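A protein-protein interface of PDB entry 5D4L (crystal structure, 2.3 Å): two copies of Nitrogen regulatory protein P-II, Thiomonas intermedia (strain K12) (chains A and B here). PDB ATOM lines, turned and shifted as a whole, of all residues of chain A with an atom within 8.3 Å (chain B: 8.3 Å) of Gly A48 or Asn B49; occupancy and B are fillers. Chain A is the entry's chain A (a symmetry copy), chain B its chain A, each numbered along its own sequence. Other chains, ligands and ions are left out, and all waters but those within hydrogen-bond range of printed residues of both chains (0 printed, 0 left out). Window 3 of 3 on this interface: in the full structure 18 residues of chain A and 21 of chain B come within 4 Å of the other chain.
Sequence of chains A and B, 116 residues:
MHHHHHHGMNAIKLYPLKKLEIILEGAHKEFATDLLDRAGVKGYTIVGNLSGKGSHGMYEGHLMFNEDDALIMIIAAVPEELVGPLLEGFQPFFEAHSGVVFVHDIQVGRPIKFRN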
ATOM      1  N   GLY A  26     -25.283  -9.152  -0.293  1.00  0.00           N
ATOM      2  CA  GLY A  26     -25.699  -7.806   0.032  1.00  0.00           C
ATOM      3  C   GLY A  26     -25.155  -7.255   1.338  1.00  0.00           C
ATOM      4  O   GLY A  26     -24.899  -6.061   1.454  1.00  0.00           O
ATOM      5  N   THR A  45     -22.807   1.519 -10.028  1.00  0.00           N
ATOM      6  CA  THR A  45     -24.232   1.253  -9.884  1.00  0.00           C
ATOM      7  C   THR A  45     -24.410  -0.136  -9.306  1.00  0.00           C
ATOM      8  O   THR A  45     -23.487  -0.962  -9.318  1.00  0.00           O
ATOM      9  CB  THR A  45     -25.008   1.380 -11.218  1.00  0.00           C
ATOM     10  OG1 THR A  45     -24.383   0.558 -12.194  1.00  0.00           O
ATOM     11  CG2 THR A  45     -25.010   2.818 -11.721  1.00  0.00           C
ATOM     12  N   ILE A  46     -25.592  -0.385  -8.761  1.00  0.00           N
ATOM     13  CA  ILE A  46     -25.835  -1.633  -8.071  1.00  0.00           C
ATOM     14  C   ILE A  46     -27.125  -2.273  -8.531  1.00  0.00           C
ATOM     15  O   ILE A  46     -28.172  -1.630  -8.514  1.00  0.00           O
ATOM     16  CB  ILE A  46     -25.885  -1.431  -6.568  1.00  0.00           C
ATOM     17  CG1 ILE A  46     -24.550  -0.824  -6.099  1.00  0.00           C
ATOM     18  CG2 ILE A  46     -26.205  -2.776  -5.865  1.00  0.00           C
ATOM     19  CD1 ILE A  46     -24.386  -0.763  -4.616  1.00  0.00           C
ATOM     20  N   VAL A  47     -27.020  -3.529  -8.969  1.00  0.00           N
ATOM     21  CA  VAL A  47     -28.180  -4.336  -9.306  1.00  0.00           C
ATOM     22  C   VAL A  47     -28.504  -5.210  -8.106  1.00  0.00           C
ATOM     23  O   VAL A  47     -27.638  -5.954  -7.632  1.00  0.00           O
ATOM     24  CB  VAL A  47     -27.950  -5.236 -10.565  1.00  0.00           C
ATOM     25  CG1 VAL A  47     -29.254  -5.910 -10.977  1.00  0.00           C
ATOM     26  CG2 VAL A  47     -27.388  -4.437 -11.742  1.00  0.00           C
ATOM     27  N   GLY A  48     -29.735  -5.121  -7.610  1.00  0.00           N
ATOM     28  CA  GLY A  48     -30.150  -5.931  -6.480  1.00  0.00           C
ATOM     29  C   GLY A  48     -30.879  -7.212  -6.879  1.00  0.00           C
ATOM     30  O   GLY A  48     -31.100  -7.471  -8.059  1.00  0.00           O
ATOM     31  N   ASN A  49     -31.244  -8.014  -5.887  1.00  0.00           N
ATOM     32  CA  ASN A  49     -32.007  -9.250  -6.105  1.00  0.00           C
ATOM     33  C   ASN A  49     -31.400 -10.245  -7.087  1.00  0.00           C
ATOM     34  O   ASN A  49     -32.087 -10.766  -7.957  1.00  0.00           O
ATOM     35  CB  ASN A  49     -33.436  -8.924  -6.554  1.00  0.00           C
ATOM     36  CG  ASN A  49     -34.452  -9.102  -5.426  1.00  0.00           C
ATOM     37  OD1 ASN A  49     -34.643 -10.210  -4.906  1.00  0.00           O
ATOM     38  ND2 ASN A  49     -35.106  -8.007  -5.040  1.00  0.00           N
ATOM     39  N   LEU A  50     -30.106 -10.484  -6.950  1.00  0.00           N
ATOM     40  CA  LEU A  50     -29.479 -11.623  -7.583  1.00  0.00           C
ATOM     41  C   LEU A  50     -29.515 -12.800  -6.620  1.00  0.00           C
ATOM     42  O   LEU A  50     -29.558 -12.624  -5.403  1.00  0.00           O
ATOM     43  CB  LEU A  50     -28.034 -11.330  -7.983  1.00  0.00           C
ATOM     44  CG  LEU A  50     -27.764 -10.655  -9.328  1.00  0.00           C
ATOM     45  CD1 LEU A  50     -28.163  -9.163  -9.330  1.00  0.00           C
ATOM     46  CD2 LEU A  50     -26.302 -10.838  -9.703  1.00  0.00           C
ATOM     47  N   SER A  51     -29.511 -13.997  -7.185  1.00  0.00           N
ATOM     48  CA  SER A  51     -29.308 -15.216  -6.435  1.00  0.00           C
ATOM     49  C   SER A  51     -28.306 -16.028  -7.224  1.00  0.00           C
ATOM     50  O   SER A  51     -27.902 -15.628  -8.317  1.00  0.00           O
ATOM     51  CB  SER A  51     -30.602 -15.988  -6.243  1.00  0.00           C
ATOM     52  OG  SER A  51     -31.189 -16.265  -7.498  1.00  0.00           O
ATOM     53  N   ALA A  70     -28.567 -13.716  -0.708  1.00  0.00           N
ATOM     54  CA  ALA A  70     -29.144 -12.551  -1.371  1.00  0.00           C
ATOM     55  C   ALA A  70     -28.001 -11.786  -1.985  1.00  0.00           C
ATOM     56  O   ALA A  70     -27.264 -11.105  -1.273  1.00  0.00           O
ATOM     57  CB  ALA A  70     -29.910 -11.684  -0.392  1.00  0.00           C
ATOM     58  N   LEU A  71     -27.825 -11.902  -3.295  1.00  0.00           N
ATOM     59  CA  LEU A  71     -26.657 -11.295  -3.913  1.00  0.00           C
ATOM     60  C   LEU A  71     -26.979  -9.955  -4.574  1.00  0.00           C
ATOM     61  O   LEU A  71     -28.130  -9.662  -4.923  1.00  0.00           O
ATOM     62  CB  LEU A  71     -26.044 -12.256  -4.924  1.00  0.00           C
ATOM     63  CG  LEU A  71     -25.723 -13.675  -4.424  1.00  0.00           C
ATOM     64  CD1 LEU A  71     -25.468 -14.571  -5.597  1.00  0.00           C
ATOM     65  CD2 LEU A  71     -24.526 -13.722  -3.444  1.00  0.00           C
ATOM     66  N   ILE A  72     -25.948  -9.132  -4.715  1.00  0.00           N
ATOM     67  CA  ILE A  72     -26.022  -7.935  -5.535  1.00  0.00           C
ATOM     68  C   ILE A  72     -24.910  -7.972  -6.569  1.00  0.00           C
ATOM     69  O   ILE A  72     -23.960  -8.738  -6.453  1.00  0.00           O
ATOM     70  CB  ILE A  72     -25.875  -6.645  -4.712  1.00  0.00           C
ATOM     71  CG1 ILE A  72     -24.529  -6.646  -3.982  1.00  0.00           C
ATOM     72  CG2 ILE A  72     -27.051  -6.477  -3.748  1.00  0.00           C
ATOM     73  CD1 ILE A  72     -24.221  -5.331  -3.254  1.00  0.00           C
ATOM     74  N   MET A  73     -25.030  -7.127  -7.577  1.00  0.00           N
ATOM     75  CA  MET A  73     -23.950  -6.915  -8.498  1.00  0.00           C
ATOM     76  C   MET A  73     -23.571  -5.458  -8.436  1.00  0.00           C
ATOM     77  O   MET A  73     -24.409  -4.586  -8.654  1.00  0.00           O
ATOM     78  CB  MET A  73     -24.345  -7.306  -9.928  1.00  0.00           C
ATOM     79  CG  MET A  73     -23.300  -6.925 -10.974  1.00  0.00           C
ATOM     80  SD  MET A  73     -23.794  -7.372 -12.649  1.00  0.00           S
ATOM     81  CE  MET A  73     -23.695  -9.151 -12.533  1.00  0.00           C
ATOM     82  N   ILE A  74     -22.308  -5.193  -8.128  1.00  0.00           N
ATOM     83  CA  ILE A  74     -21.791  -3.841  -8.196  1.00  0.00           C
ATOM     84  C   ILE A  74     -21.071  -3.653  -9.537  1.00  0.00           C
ATOM     85  O   ILE A  74     -20.238  -4.467  -9.929  1.00  0.00           O
ATOM     86  CB  ILE A  74     -20.863  -3.559  -7.011  1.00  0.00           C
ATOM     87  CG1 ILE A  74     -21.606  -3.885  -5.711  1.00  0.00           C
ATOM     88  CG2 ILE A  74     -20.355  -2.123  -7.041  1.00  0.00           C
ATOM     89  CD1 ILE A  74     -20.836  -3.567  -4.462  1.00  0.00           C
ATOM     90  N   GLY B  26     -35.575   5.711 -14.140  1.00  0.00           N
ATOM     91  CA  GLY B  26     -36.771   5.072 -14.639  1.00  0.00           C
ATOM     92  C   GLY B  26     -37.781   6.000 -15.289  1.00  0.00           C
ATOM     93  O   GLY B  26     -38.469   5.615 -16.229  1.00  0.00           O
ATOM     94  N   ILE B  46     -35.061  -4.862 -20.189  1.00  0.00           N
ATOM     95  CA  ILE B  46     -34.895  -3.867 -19.153  1.00  0.00           C
ATOM     96  C   ILE B  46     -34.721  -4.510 -17.797  1.00  0.00           C
ATOM     97  O   ILE B  46     -35.543  -5.330 -17.394  1.00  0.00           O
ATOM     98  CB  ILE B  46     -36.076  -2.915 -19.108  1.00  0.00           C
ATOM     99  CG1 ILE B  46     -36.218  -2.226 -20.478  1.00  0.00           C
ATOM    100  CG2 ILE B  46     -35.892  -1.900 -17.950  1.00  0.00           C
ATOM    101  CD1 ILE B  46     -37.214  -1.113 -20.510  1.00  0.00           C
ATOM    102  N   VAL B  47     -33.627  -4.148 -17.124  1.00  0.00           N
ATOM    103  CA  VAL B  47     -33.387  -4.558 -15.751  1.00  0.00           C
ATOM    104  C   VAL B  47     -33.828  -3.421 -14.843  1.00  0.00           C
ATOM    105  O   VAL B  47     -33.359  -2.288 -14.997  1.00  0.00           O
ATOM    106  CB  VAL B  47     -31.885  -4.899 -15.472  1.00  0.00           C
ATOM    107  CG1 VAL B  47     -31.730  -5.497 -14.079  1.00  0.00           C
ATOM    108  CG2 VAL B  47     -31.317  -5.863 -16.516  1.00  0.00           C
ATOM    109  N   GLY B  48     -34.726  -3.713 -13.905  1.00  0.00           N
ATOM    110  CA  GLY B  48     -35.195  -2.705 -12.974  1.00  0.00           C
ATOM    111  C   GLY B  48     -34.453  -2.712 -11.640  1.00  0.00           C
ATOM    112  O   GLY B  48     -33.572  -3.536 -11.411  1.00  0.00           O
ATOM    113  N   ASN B  49     -34.810  -1.781 -10.763  1.00  0.00           N
ATOM    114  CA  ASN B  49     -34.235  -1.697  -9.415  1.00  0.00           C
ATOM    115  C   ASN B  49     -32.715  -1.609  -9.343  1.00  0.00           C
ATOM    116  O   ASN B  49     -32.082  -2.310  -8.562  1.00  0.00           O
ATOM    117  CB  ASN B  49     -34.700  -2.881  -8.560  1.00  0.00           C
ATOM    118  CG  ASN B  49     -35.790  -2.483  -7.564  1.00  0.00           C
ATOM    119  OD1 ASN B  49     -35.567  -1.652  -6.671  1.00  0.00           O
ATOM    120  ND2 ASN B  49     -36.975  -3.070  -7.716  1.00  0.00           N
ATOM    121  N   LEU B  50     -32.139  -0.758 -10.176  1.00  0.00           N
ATOM    122  CA  LEU B  50     -30.767  -0.339  -9.997  1.00  0.00           C
ATOM    123  C   LEU B  50     -30.748   0.919  -9.140  1.00  0.00           C
ATOM    124  O   LEU B  50     -31.713   1.682  -9.110  1.00  0.00           O
ATOM    125  CB  LEU B  50     -30.076  -0.062 -11.333  1.00  0.00           C
ATOM    126  CG  LEU B  50     -29.438  -1.229 -12.086  1.00  0.00           C
ATOM    127  CD1 LEU B  50     -30.487  -2.168 -12.720  1.00  0.00           C
ATOM    128  CD2 LEU B  50     -28.473  -0.690 -13.131  1.00  0.00           C
ATOM    129  N   SER B  51     -29.642   1.111  -8.439  1.00  0.00           N
ATOM    130  CA  SER B  51     -29.352   2.354  -7.759  1.00  0.00           C
ATOM    131  C   SER B  51     -27.914   2.683  -8.090  1.00  0.00           C
ATOM    132  O   SER B  51     -27.231   1.900  -8.750  1.00  0.00           O
ATOM    133  CB  SER B  51     -29.553   2.241  -6.258  1.00  0.00           C
ATOM    134  OG  SER B  51     -28.758   1.192  -5.743  1.00  0.00           O
ATOM    135  N   GLY B  52     -27.435   3.832  -7.648  1.00  0.00           N
ATOM    136  CA  GLY B  52     -26.119   4.233  -8.080  1.00  0.00           C
ATOM    137  C   GLY B  52     -25.599   5.413  -7.333  1.00  0.00           C
ATOM    138  O   GLY B  52     -26.278   5.976  -6.484  1.00  0.00           O
ATOM    139  N   ASP B  69     -31.887   8.035  -6.728  1.00  0.00           N
ATOM    140  CA  ASP B  69     -32.252   7.718  -8.097  1.00  0.00           C
ATOM    141  C   ASP B  69     -32.717   6.267  -8.207  1.00  0.00           C
ATOM    142  O   ASP B  69     -32.013   5.342  -7.778  1.00  0.00           O
ATOM    143  CB  ASP B  69     -31.077   7.943  -9.037  1.00  0.00           C
ATOM    144  CG  ASP B  69     -30.782   9.406  -9.271  1.00  0.00           C
ATOM    145  OD1 ASP B  69     -31.727  10.237  -9.250  1.00  0.00           O
ATOM    146  OD2 ASP B  69     -29.595   9.708  -9.508  1.00  0.00           O
ATOM    147  N   ALA B  70     -33.907   6.073  -8.765  1.00  0.00           N
ATOM    148  CA  ALA B  70     -34.377   4.736  -9.115  1.00  0.00           C
ATOM    149  C   ALA B  70     -33.943   4.477 -10.534  1.00  0.00           C
ATOM    150  O   ALA B  70     -34.541   5.009 -11.468  1.00  0.00           O
ATOM    151  CB  ALA B  70     -35.884   4.632  -8.984  1.00  0.00           C
ATOM    152  N   LEU B  71     -32.895   3.683 -10.712  1.00  0.00           N
ATOM    153  CA  LEU B  71     -32.353   3.511 -12.051  1.00  0.00           C
ATOM    154  C   LEU B  71     -32.825   2.213 -12.708  1.00  0.00           C
ATOM    155  O   LEU B  71     -33.227   1.254 -12.037  1.00  0.00           O
ATOM    156  CB  LEU B  71     -30.831   3.564 -12.008  1.00  0.00           C
ATOM    157  CG  LEU B  71     -30.200   4.785 -11.315  1.00  0.00           C
ATOM    158  CD1 LEU B  71     -28.751   4.515 -11.051  1.00  0.00           C
ATOM    159  CD2 LEU B  71     -30.363   6.096 -12.120  1.00  0.00           C
ATOM    160  N   ILE B  72     -32.797   2.208 -14.034  1.00  0.00           N
ATOM    161  CA  ILE B  72     -32.973   0.991 -14.805  1.00  0.00           C
ATOM    162  C   ILE B  72     -31.782   0.813 -15.731  1.00  0.00           C
ATOM    163  O   ILE B  72     -31.019   1.742 -15.970  1.00  0.00           O
ATOM    164  CB  ILE B  72     -34.251   1.011 -15.660  1.00  0.00           C
ATOM    165  CG1 ILE B  72     -34.207   2.193 -16.631  1.00  0.00           C
ATOM    166  CG2 ILE B  72     -35.497   1.041 -14.773  1.00  0.00           C
ATOM    167  CD1 ILE B  72     -35.369   2.212 -17.633  1.00  0.00           C
ATOM    168  N   MET B  73     -31.637  -0.388 -16.262  1.00  0.00           N
ATOM    169  CA  MET B  73     -30.685  -0.624 -17.311  1.00  0.00           C
ATOM    170  C   MET B  73     -31.441  -1.117 -18.517  1.00  0.00           C
ATOM    171  O   MET B  73     -32.152  -2.118 -18.441  1.00  0.00           O
ATOM    172  CB  MET B  73     -29.623  -1.647 -16.888  1.00  0.00           C
ATOM    173  CG  MET B  73     -28.700  -2.073 -18.027  1.00  0.00           C
ATOM    174  SD  MET B  73     -27.476  -3.293 -17.513  1.00  0.00           S
ATOM    175  CE  MET B  73     -26.456  -2.277 -16.456  1.00  0.00           C
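O of Ser B51 lies within hydrogen-bond range of N of Ile A46, 2.8 Å away.
Gly A48 touches one residue of chain B.
Of chain A, only Ile A46 (3.97 Å) and Gly A48 (3.8 Å) come within 4 Å of Asn B49.
Of the printed residues of chain A, Ser B51 touches Thr A45 and Ile A46.
Printed residues of chain B within 4 Å of Val A47: Val B47 (3.99 Å) and Leu B50 (3.8 Å).
Printed residues of chain B within 4 Å of Thr A45: Ser B51 (3.3 Å) and Gly B52 (3.96 Å).
Of the printed residues of chain A, Val B47 touches Val A47 (3.99 Å).
Of the printed residues of chain A, Gly B52 touches Thr A45 (3.96 Å).
Ala A70 touches none of the printed residues of chain B.
Ile A72 touches none of the printed residues of chain B.
The nearest residue of chain B that does not touch Gly A48 is Leu B50 (5.4 Å).
The nearest residue of chain A that does not touch Asn B49 is Val A47 (4.5 Å).
The nearest printed residue of chain A that does not touch Ser B51 is Val A47 (5.4 Å).
O of Leu B50 sits at hydrogen-bond distance from N of Leu B71, 2.8 Å away.
The backbone carbonyl oxygen (O) of Met B73 is in hydrogen-bond range of the backbone NH (N) of Val B47, 2.8 Å away.
N of Val A47 sits at hydrogen-bond distance from O of Met A73, 2.8 Å away.
Hydrophobic or aromatic side chains of chain B within 4 Å of the printed part of chain A: Val B47 and Leu B50.
Of the 13 printed residues of chain A, 4 touch a printed residue of chain B.
Hydrophobic or aromatic side chains of chain A within 4 Å of the printed part of chain B: Ile A46 and Val A47.
Among the printed residues, 8 pairs touch across the chains.
Among the printed residues, merely in contact across the chains: Thr A45 with Ser B51 (3.3 Å), Thr A45 with Gly B52 (3.96 Å), Ile A46 with Asn B49 (3.97 Å), Ile A46 with Leu B50 (3.3 Å), Val A47 with Val B47 (3.99 Å), Val A47 with Leu B50 (3.8 Å) and Gly A48 with Asn B49 (3.8 Å).
Ile A46 touches Asn B49, but with the chains exchanged Asn A49 does not touch Ile B46 (11.4 Å).
Ile A46 touches Leu B50, but with the chains exchanged Leu A50 does not touch Ile B46 (11.6 Å).
Ile A46 touches Ser B51, but with the chains exchanged Ser A51 does not touch Ile B46 (14.7 Å).
Val A47 touches Leu B50, but with the chains exchanged Leu A50 does not touch Val B47 (7.0 Å).
Of the 8 pairs that touch across the chains among the printed residues, 1 has its exchanged pair printed and touching as well.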
